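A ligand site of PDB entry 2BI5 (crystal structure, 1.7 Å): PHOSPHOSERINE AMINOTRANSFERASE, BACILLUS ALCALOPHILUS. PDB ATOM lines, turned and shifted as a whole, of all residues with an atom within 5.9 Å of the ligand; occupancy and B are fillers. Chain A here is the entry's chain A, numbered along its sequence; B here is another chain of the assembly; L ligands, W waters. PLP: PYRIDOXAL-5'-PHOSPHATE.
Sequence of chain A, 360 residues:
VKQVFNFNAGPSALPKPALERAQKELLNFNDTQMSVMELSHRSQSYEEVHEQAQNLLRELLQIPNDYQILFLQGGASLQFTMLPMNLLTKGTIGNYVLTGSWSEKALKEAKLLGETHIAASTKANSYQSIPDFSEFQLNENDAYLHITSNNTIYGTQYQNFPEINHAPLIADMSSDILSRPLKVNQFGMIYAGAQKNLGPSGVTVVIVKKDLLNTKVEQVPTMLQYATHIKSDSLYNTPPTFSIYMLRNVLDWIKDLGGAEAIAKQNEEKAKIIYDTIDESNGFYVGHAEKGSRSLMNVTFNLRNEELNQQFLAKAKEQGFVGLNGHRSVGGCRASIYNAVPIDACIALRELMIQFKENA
CA of Gly 75 touches O3P of the ligand, 3.2 Å away. Phe 80 touches the ligand (CZ to C6, 3.7 Å). Thr 148 touches the ligand (CG2 to C2A, 3.96 Å). O of Asn 150 touches C2A of the ligand (3.8 Å). Ser 174 touches the ligand (CB to C2, 3.5 Å). Ser 175 touches the ligand (OG to O3, 3.9 Å). Hydrophobic or aromatic side chains within 4 Å of the ligand: Ala 76, Phe 80 and Trp 102. Within 4 Å of the ligand: Gly 75, Ala 76, Ser 77, Phe 80, Trp 102, Thr 148, Asn 150, Thr 152, Asp 172, Ser 174, Ser 175, Gln 195, Lys 196, Asn 237 of chain B and Thr 238 of chain B. The nearest printed residue that does not touch the ligand is Gly 74 (4.5 Å).
Water W3 lies within hydrogen-bond range of O of Thr 238 of chain B (2.7 Å), O3P of the ligand (2.7 Å) and NE2 of Gln 73 of chain B (3.1 Å). Water W1 lies within hydrogen-bond range of O4P of the ligand (2.9 Å), OG of Ser 174 (2.9 Å) and N of Gly 193 (3.0 Å).
O of Thr 238 of chain B sits at hydrogen-bond distance from NE2 of Gln 73 of chain B. N of Gly 193 lies within hydrogen-bond range of OG of Ser 174. The side-chain amide nitrogen (ND2) of Asn 237 of chain B sits at hydrogen-bond distance from the backbone carbonyl oxygen (O) of Gly 74. OG1 of Thr 152 is in hydrogen-bond range of OG of Ser 175 (2.7 Å). The side-chain hydroxyl of Thr 238 of chain B is in hydrogen-bond range of the side-chain amide nitrogen of Gln 195, at 3.2 Å. The side-chain hydroxyl of Ser 175 sits at hydrogen-bond distance from the side-chain amide oxygen of Asn 150 (2.9 Å). The side-chain carboxylate (OD1) of Asp 172 sits at hydrogen-bond distance from the side-chain hydroxyl (OG) of Ser 174, 2.8 Å away. The backbone NH (N) of Gly 75 sits close to the side-chain hydroxyl (OG1) of Thr 204, 3.1 Å away.
O3 of the ligand is in hydrogen-bond range of OG1 of Thr 152 (2.5 Å). An oxygen (O3P) of the ligand is in hydrogen-bond range of the backbone NH (N) of Ala 76 (3.2 Å). NE2 of Gln 195 is in hydrogen-bond range of O3P of the ligand (2.8 Å). NE1 of Trp 102 sits close to O3 of the ligand. An oxygen (O2P) of the ligand lies within hydrogen-bond range of the backbone NH (N) of Ser 77, at 2.8 Å. The side-chain carboxylate of Asp 172 lies within hydrogen-bond range of a nitrogen (N1) of the ligand (2.7 Å). OG of Ser 77 is in hydrogen-bond range of O2P of the ligand, 2.7 Å away. O1P of the ligand lies within hydrogen-bond range of OG1 of Thr 238 of chain B, at 2.7 Å. N of Thr 238 of chain B sits at hydrogen-bond distance from O1P of the ligand (3.0 Å). The side-chain amide nitrogen (ND2) of Asn 237 of chain B sits at hydrogen-bond distance from an oxygen (O2P) of the ligand (2.9 Å). A carbon (C4A) of the ligand is covalently linked to the side-chain amino group (NZ) of Lys 196.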
ATOM      1  N   ALA A   9      16.056 -10.205  17.300  1.00  0.00           N
ATOM      2  CA  ALA A   9      16.324 -11.169  16.256  1.00  0.00           C
ATOM      3  C   ALA A   9      15.236 -11.284  15.194  1.00  0.00           C
ATOM      4  O   ALA A   9      15.413 -12.006  14.199  1.00  0.00           O
ATOM      5  CB  ALA A   9      16.588 -12.558  16.883  1.00  0.00           C
ATOM      6  N   GLY A  74       2.191 -14.833   5.169  1.00  0.00           N
ATOM      7  CA  GLY A  74       2.314 -16.172   5.725  1.00  0.00           C
ATOM      8  C   GLY A  74       3.680 -16.480   6.313  1.00  0.00           C
ATOM      9  O   GLY A  74       3.853 -17.489   7.011  1.00  0.00           O
ATOM     10  N   GLY A  75       4.636 -15.604   6.039  1.00  0.00           N
ATOM     11  CA  GLY A  75       5.956 -15.800   6.657  1.00  0.00           C
ATOM     12  C   GLY A  75       6.756 -16.864   5.909  1.00  0.00           C
ATOM     13  O   GLY A  75       6.294 -17.530   4.991  1.00  0.00           O
ATOM     14  N   ALA A  76       8.031 -16.982   6.332  1.00  0.00           N
ATOM     15  CA  ALA A  76       8.854 -18.047   5.733  1.00  0.00           C
ATOM     16  C   ALA A  76       8.250 -19.401   6.035  1.00  0.00           C
ATOM     17  O   ALA A  76       8.321 -20.374   5.282  1.00  0.00           O
ATOM     18  CB  ALA A  76      10.275 -17.932   6.252  1.00  0.00           C
ATOM     19  N   SER A  77       7.632 -19.458   7.218  1.00  0.00           N
ATOM     20  CA  SER A  77       7.035 -20.733   7.643  1.00  0.00           C
ATOM     21  C   SER A  77       6.033 -21.240   6.629  1.00  0.00           C
ATOM     22  O   SER A  77       5.998 -22.451   6.368  1.00  0.00           O
ATOM     23  CB  SER A  77       6.398 -20.619   9.032  1.00  0.00           C
ATOM     24  OG  SER A  77       7.419 -20.376   9.992  1.00  0.00           O
ATOM     25  N   LEU A  78       5.233 -20.355   6.043  1.00  0.00           N
ATOM     26  CA  LEU A  78       4.304 -20.821   5.022  1.00  0.00           C
ATOM     27  C   LEU A  78       5.061 -21.308   3.781  1.00  0.00           C
ATOM     28  O   LEU A  78       4.632 -22.230   3.095  1.00  0.00           O
ATOM     29  CB  LEU A  78       3.294 -19.748   4.600  1.00  0.00           C
ATOM     30  CG  LEU A  78       2.239 -20.259   3.611  1.00  0.00           C
ATOM     31  CD1 LEU A  78       1.548 -21.491   4.197  1.00  0.00           C
ATOM     32  CD2 LEU A  78       1.251 -19.171   3.247  1.00  0.00           C
ATOM     33  N   PHE A  80       7.782 -22.932   3.805  1.00  0.00           N
ATOM     34  CA  PHE A  80       8.218 -24.296   4.067  1.00  0.00           C
ATOM     35  C   PHE A  80       7.249 -25.331   3.481  1.00  0.00           C
ATOM     36  O   PHE A  80       7.667 -26.405   3.028  1.00  0.00           O
ATOM     37  CB  PHE A  80       8.354 -24.550   5.562  1.00  0.00           C
ATOM     38  CG  PHE A  80       9.428 -23.781   6.309  1.00  0.00           C
ATOM     39  CD1 PHE A  80       9.376 -23.690   7.693  1.00  0.00           C
ATOM     40  CD2 PHE A  80      10.469 -23.147   5.623  1.00  0.00           C
ATOM     41  CE1 PHE A  80      10.328 -22.984   8.426  1.00  0.00           C
ATOM     42  CE2 PHE A  80      11.437 -22.482   6.343  1.00  0.00           C
ATOM     43  CZ  PHE A  80      11.372 -22.390   7.721  1.00  0.00           C
ATOM     44  N   TRP A 102      16.023 -23.926  11.667  1.00  0.00           N
ATOM     45  CA  TRP A 102      15.143 -23.535  10.557  1.00  0.00           C
ATOM     46  C   TRP A 102      15.264 -24.527   9.399  1.00  0.00           C
ATOM     47  O   TRP A 102      14.268 -24.827   8.730  1.00  0.00           O
ATOM     48  CB  TRP A 102      15.392 -22.101  10.095  1.00  0.00           C
ATOM     49  CG  TRP A 102      14.983 -21.120  11.157  1.00  0.00           C
ATOM     50  CD1 TRP A 102      15.774 -20.256  11.862  1.00  0.00           C
ATOM     51  CD2 TRP A 102      13.647 -20.920  11.625  1.00  0.00           C
ATOM     52  NE1 TRP A 102      15.014 -19.531  12.739  1.00  0.00           N
ATOM     53  CE2 TRP A 102      13.695 -19.915  12.617  1.00  0.00           C
ATOM     54  CE3 TRP A 102      12.411 -21.493  11.289  1.00  0.00           C
ATOM     55  CZ2 TRP A 102      12.563 -19.466  13.293  1.00  0.00           C
ATOM     56  CZ3 TRP A 102      11.292 -21.045  11.971  1.00  0.00           C
ATOM     57  CH2 TRP A 102      11.359 -20.047  12.954  1.00  0.00           C
ATOM     58  N   THR A 148      19.547 -23.286   3.912  1.00  0.00           N
ATOM     59  CA  THR A 148      19.290 -22.133   4.777  1.00  0.00           C
ATOM     60  C   THR A 148      20.562 -21.283   4.793  1.00  0.00           C
ATOM     61  O   THR A 148      21.541 -21.655   5.442  1.00  0.00           O
ATOM     62  CB  THR A 148      18.889 -22.584   6.178  1.00  0.00           C
ATOM     63  OG1 THR A 148      17.896 -23.626   6.035  1.00  0.00           O
ATOM     64  CG2 THR A 148      18.273 -21.438   6.980  1.00  0.00           C
ATOM     65  N   ASN A 150      21.523 -18.443   6.104  1.00  0.00           N
ATOM     66  CA  ASN A 150      21.917 -17.968   7.432  1.00  0.00           C
ATOM     67  C   ASN A 150      21.086 -18.663   8.504  1.00  0.00           C
ATOM     68  O   ASN A 150      19.843 -18.590   8.508  1.00  0.00           O
ATOM     69  CB  ASN A 150      21.787 -16.439   7.541  1.00  0.00           C
ATOM     70  CG  ASN A 150      22.373 -15.902   8.835  1.00  0.00           C
ATOM     71  OD1 ASN A 150      21.651 -15.634   9.806  1.00  0.00           O
ATOM     72  ND2 ASN A 150      23.679 -15.727   8.906  1.00  0.00           N
ATOM     73  N   ASN A 151      21.772 -19.368   9.397  1.00  0.00           N
ATOM     74  CA  ASN A 151      21.114 -20.190  10.414  1.00  0.00           C
ATOM     75  C   ASN A 151      20.930 -19.356  11.672  1.00  0.00           C
ATOM     76  O   ASN A 151      21.795 -19.310  12.534  1.00  0.00           O
ATOM     77  CB  ASN A 151      21.938 -21.473  10.616  1.00  0.00           C
ATOM     78  CG  ASN A 151      22.175 -22.151   9.280  1.00  0.00           C
ATOM     79  OD1 ASN A 151      21.286 -22.841   8.766  1.00  0.00           O
ATOM     80  ND2 ASN A 151      23.334 -21.959   8.692  1.00  0.00           N
ATOM     81  N   THR A 152      19.777 -18.682  11.705  1.00  0.00           N
ATOM     82  CA  THR A 152      19.505 -17.604  12.627  1.00  0.00           C
ATOM     83  C   THR A 152      19.749 -17.957  14.082  1.00  0.00           C
ATOM     84  O   THR A 152      20.163 -17.141  14.899  1.00  0.00           O
ATOM     85  CB  THR A 152      18.029 -17.163  12.454  1.00  0.00           C
ATOM     86  OG1 THR A 152      17.732 -17.310  11.073  1.00  0.00           O
ATOM     87  CG2 THR A 152      17.863 -15.695  12.815  1.00  0.00           C
ATOM     88  N   ASP A 172      16.289 -20.532   1.880  1.00  0.00           N
ATOM     89  CA  ASP A 172      15.671 -19.715   2.915  1.00  0.00           C
ATOM     90  C   ASP A 172      16.718 -18.680   3.338  1.00  0.00           C
ATOM     91  O   ASP A 172      17.636 -19.008   4.110  1.00  0.00           O
ATOM     92  CB  ASP A 172      15.226 -20.578   4.070  1.00  0.00           C
ATOM     93  CG  ASP A 172      14.689 -19.821   5.264  1.00  0.00           C
ATOM     94  OD1 ASP A 172      14.611 -18.568   5.180  1.00  0.00           O
ATOM     95  OD2 ASP A 172      14.343 -20.490   6.271  1.00  0.00           O
ATOM     96  N   MET A 173      16.548 -17.453   2.829  1.00  0.00           N
ATOM     97  CA  MET A 173      17.474 -16.376   3.187  1.00  0.00           C
ATOM     98  C   MET A 173      16.855 -15.357   4.138  1.00  0.00           C
ATOM     99  O   MET A 173      17.298 -14.218   4.121  1.00  0.00           O
ATOM    100  CB  MET A 173      17.956 -15.668   1.925  1.00  0.00           C
ATOM    101  CG  MET A 173      18.762 -16.597   1.007  1.00  0.00           C
ATOM    102  SD  MET A 173      19.535 -15.614  -0.298  1.00  0.00           S
ATOM    103  CE  MET A 173      20.445 -16.914  -1.166  1.00  0.00           C
ATOM    104  N   SER A 174      15.886 -15.771   4.938  1.00  0.00           N
ATOM    105  CA  SER A 174      15.190 -14.871   5.867  1.00  0.00           C
ATOM    106  C   SER A 174      16.136 -13.976   6.637  1.00  0.00           C
ATOM    107  O   SER A 174      15.894 -12.761   6.717  1.00  0.00           O
ATOM    108  CB  SER A 174      14.352 -15.695   6.846  1.00  0.00           C
ATOM    109  OG  SER A 174      13.293 -16.372   6.194  1.00  0.00           O
ATOM    110  N   SER A 175      17.237 -14.529   7.192  1.00  0.00           N
ATOM    111  CA  SER A 175      18.010 -13.643   8.073  1.00  0.00           C
ATOM    112  C   SER A 175      19.267 -13.076   7.443  1.00  0.00           C
ATOM    113  O   SER A 175      20.032 -12.452   8.179  1.00  0.00           O
ATOM    114  CB  SER A 175      18.343 -14.351   9.402  1.00  0.00           C
ATOM    115  OG  SER A 175      18.816 -15.672   9.188  1.00  0.00           O
ATOM    116  N   TYR A 191      13.642 -17.271  -0.712  1.00  0.00           N
ATOM    117  CA  TYR A 191      12.546 -16.625   0.049  1.00  0.00           C
ATOM    118  C   TYR A 191      13.059 -16.101   1.375  1.00  0.00           C
ATOM    119  O   TYR A 191      14.063 -16.561   1.898  1.00  0.00           O
ATOM    120  CB  TYR A 191      11.380 -17.585   0.206  1.00  0.00           C
ATOM    121  CG  TYR A 191      11.651 -18.840   0.991  1.00  0.00           C
ATOM    122  CD1 TYR A 191      11.441 -18.902   2.360  1.00  0.00           C
ATOM    123  CD2 TYR A 191      12.127 -19.998   0.360  1.00  0.00           C
ATOM    124  CE1 TYR A 191      11.687 -20.049   3.080  1.00  0.00           C
ATOM    125  CE2 TYR A 191      12.372 -21.163   1.092  1.00  0.00           C
ATOM    126  CZ  TYR A 191      12.144 -21.182   2.447  1.00  0.00           C
ATOM    127  OH  TYR A 191      12.386 -22.308   3.198  1.00  0.00           O
ATOM    128  N   GLY A 193      11.198 -14.096   5.035  1.00  0.00           N
ATOM    129  CA  GLY A 193      10.280 -13.198   5.750  1.00  0.00           C
ATOM    130  C   GLY A 193      10.980 -11.844   5.791  1.00  0.00           C
ATOM    131  O   GLY A 193      12.197 -11.703   5.984  1.00  0.00           O
ATOM    132  N   GLN A 195      10.881  -9.507   8.047  1.00  0.00           N
ATOM    133  CA  GLN A 195      11.077  -8.888   9.355  1.00  0.00           C
ATOM    134  C   GLN A 195      12.485  -9.043   9.901  1.00  0.00           C
ATOM    135  O   GLN A 195      12.797  -8.576  11.005  1.00  0.00           O
ATOM    136  CB  GLN A 195      10.102  -9.478  10.377  1.00  0.00           C
ATOM    137  CG  GLN A 195      10.366 -10.957  10.665  1.00  0.00           C
ATOM    138  CD  GLN A 195       9.607 -11.882   9.743  1.00  0.00           C
ATOM    139  OE1 GLN A 195       9.147 -11.526   8.652  1.00  0.00           O
ATOM    140  NE2 GLN A 195       9.472 -13.141  10.169  1.00  0.00           N
ATOM    141  N   LYS A 196      13.404  -9.690   9.180  1.00  0.00           N
ATOM    142  CA  LYS A 196      14.732  -9.681   9.843  1.00  0.00           C
ATOM    143  C   LYS A 196      15.635  -8.645   9.220  1.00  0.00           C
ATOM    144  O   LYS A 196      16.309  -7.846   9.868  1.00  0.00           O
ATOM    145  CB  LYS A 196      15.368 -11.076   9.795  1.00  0.00           C
ATOM    146  CG  LYS A 196      14.357 -12.176  10.082  1.00  0.00           C
ATOM    147  CD  LYS A 196      14.948 -13.221  11.020  1.00  0.00           C
ATOM    148  CE  LYS A 196      13.870 -13.825  11.890  1.00  0.00           C
ATOM    149  NZ  LYS A 196      13.697 -15.281  11.646  1.00  0.00           N
ATOM    150  N   THR A 204       6.423 -11.593   3.002  1.00  0.00           N
ATOM    151  CA  THR A 204       7.480 -12.532   2.694  1.00  0.00           C
ATOM    152  C   THR A 204       7.937 -12.303   1.257  1.00  0.00           C
ATOM    153  O   THR A 204       7.092 -12.319   0.362  1.00  0.00           O
ATOM    154  CB  THR A 204       6.979 -13.977   2.886  1.00  0.00           C
ATOM    155  OG1 THR A 204       6.722 -14.177   4.278  1.00  0.00           O
ATOM    156  CG2 THR A 204       8.048 -14.974   2.471  1.00  0.00           C
ATOM    157  N   TYR A 338      21.659  -7.330  12.032  1.00  0.00           N
ATOM    158  CA  TYR A 338      21.154  -7.133  10.676  1.00  0.00           C
ATOM    159  C   TYR A 338      21.538  -5.770  10.111  1.00  0.00           C
ATOM    160  O   TYR A 338      22.054  -4.945  10.865  1.00  0.00           O
ATOM    161  CB  TYR A 338      19.622  -7.251  10.698  1.00  0.00           C
ATOM    162  CG  TYR A 338      19.137  -8.573  11.239  1.00  0.00           C
ATOM    163  CD1 TYR A 338      18.350  -8.605  12.385  1.00  0.00           C
ATOM    164  CD2 TYR A 338      19.454  -9.763  10.601  1.00  0.00           C
ATOM    165  CE1 TYR A 338      17.886  -9.804  12.903  1.00  0.00           C
ATOM    166  CE2 TYR A 338      18.990 -10.961  11.119  1.00  0.00           C
ATOM    167  CZ  TYR A 338      18.214 -10.993  12.258  1.00  0.00           C
ATOM    168  OH  TYR A 338      17.748 -12.181  12.784  1.00  0.00           O
ATOM    169  N   HIS B  41       8.379 -10.463  18.430  1.00  0.00           N
ATOM    170  CA  HIS B  41       7.029 -10.922  18.743  1.00  0.00           C
ATOM    171  C   HIS B  41       7.018 -11.761  20.008  1.00  0.00           C
ATOM    172  O   HIS B  41       5.969 -12.136  20.526  1.00  0.00           O
ATOM    173  CB  HIS B  41       6.445 -11.700  17.570  1.00  0.00           C
ATOM    174  CG  HIS B  41       7.223 -12.928  17.212  1.00  0.00           C
ATOM    175  ND1 HIS B  41       8.532 -12.902  16.786  1.00  0.00           N
ATOM    176  CD2 HIS B  41       6.839 -14.230  17.220  1.00  0.00           C
ATOM    177  CE1 HIS B  41       8.941 -14.139  16.551  1.00  0.00           C
ATOM    178  NE2 HIS B  41       7.924 -14.971  16.798  1.00  0.00           N
ATOM    179  N   GLN B  73      -2.360 -14.760   8.865  1.00  0.00           N
ATOM    180  CA  GLN B  73      -2.024 -14.087   7.616  1.00  0.00           C
ATOM    181  C   GLN B  73      -2.728 -14.793   6.467  1.00  0.00           C
ATOM    182  O   GLN B  73      -3.251 -15.896   6.693  1.00  0.00           O
ATOM    183  CB  GLN B  73      -0.504 -14.132   7.390  1.00  0.00           C
ATOM    184  CG  GLN B  73       0.301 -13.387   8.473  1.00  0.00           C
ATOM    185  CD  GLN B  73       1.793 -13.409   8.116  1.00  0.00           C
ATOM    186  OE1 GLN B  73       2.184 -12.798   7.127  1.00  0.00           O
ATOM    187  NE2 GLN B  73       2.579 -14.120   8.930  1.00  0.00           N
ATOM    188  N   ASN B 237       4.391 -18.735  14.435  1.00  0.00           N
ATOM    189  CA  ASN B 237       5.469 -18.046  13.689  1.00  0.00           C
ATOM    190  C   ASN B 237       5.273 -16.553  13.905  1.00  0.00           C
ATOM    191  O   ASN B 237       4.495 -16.108  14.750  1.00  0.00           O
ATOM    192  CB  ASN B 237       5.520 -18.419  12.222  1.00  0.00           C
ATOM    193  CG  ASN B 237       4.411 -17.850  11.377  1.00  0.00           C
ATOM    194  OD1 ASN B 237       3.275 -17.709  11.839  1.00  0.00           O
ATOM    195  ND2 ASN B 237       4.790 -17.521  10.149  1.00  0.00           N
ATOM    196  N   THR B 238       6.005 -15.746  13.174  1.00  0.00           N
ATOM    197  CA  THR B 238       5.967 -14.306  13.423  1.00  0.00           C
ATOM    198  C   THR B 238       4.625 -13.755  12.940  1.00  0.00           C
ATOM    199  O   THR B 238       4.324 -13.882  11.754  1.00  0.00           O
ATOM    200  CB  THR B 238       7.115 -13.585  12.704  1.00  0.00           C
ATOM    201  OG1 THR B 238       8.378 -14.224  12.996  1.00  0.00           O
ATOM    202  CG2 THR B 238       7.227 -12.136  13.173  1.00  0.00           C
HETATM  203  N1  PLP L   1      13.577 -19.106   8.474  1.00  0.00           N
HETATM  204  C2  PLP L   1      14.593 -18.388   9.048  1.00  0.00           C
HETATM  205  C2A PLP L   1      16.055 -18.605   8.627  1.00  0.00           C
HETATM  206  C3  PLP L   1      14.311 -17.492  10.034  1.00  0.00           C
HETATM  207  O3  PLP L   1      15.351 -16.804  10.596  1.00  0.00           O
HETATM  208  C4  PLP L   1      13.007 -17.355  10.464  1.00  0.00           C
HETATM  209  C4A PLP L   1      12.621 -16.221  11.443  1.00  0.00           C
HETATM  210  C5  PLP L   1      11.987 -18.059   9.871  1.00  0.00           C
HETATM  211  C6  PLP L   1      12.276 -18.981   8.895  1.00  0.00           C
HETATM  212  C5A PLP L   1      10.528 -17.895  10.335  1.00  0.00           C
HETATM  213  O4P PLP L   1       9.856 -16.877   9.607  1.00  0.00           O
HETATM  214  P   PLP L   1       8.316 -16.559   9.909  1.00  0.00           P
HETATM  215  O1P PLP L   1       8.274 -16.361  11.369  1.00  0.00           O
HETATM  216  O2P PLP L   1       7.619 -17.777   9.427  1.00  0.00           O
HETATM  217  O3P PLP L   1       8.039 -15.353   9.105  1.00  0.00           O
HETATM  218  O   HOH W   1      11.311 -15.129   7.889  1.00  0.00           O
HETATM  219  O   HOH W   2       8.684 -18.021  13.481  1.00  0.00           O
HETATM  220  O   HOH W   3       5.618 -14.172   9.409  1.00  0.00           O
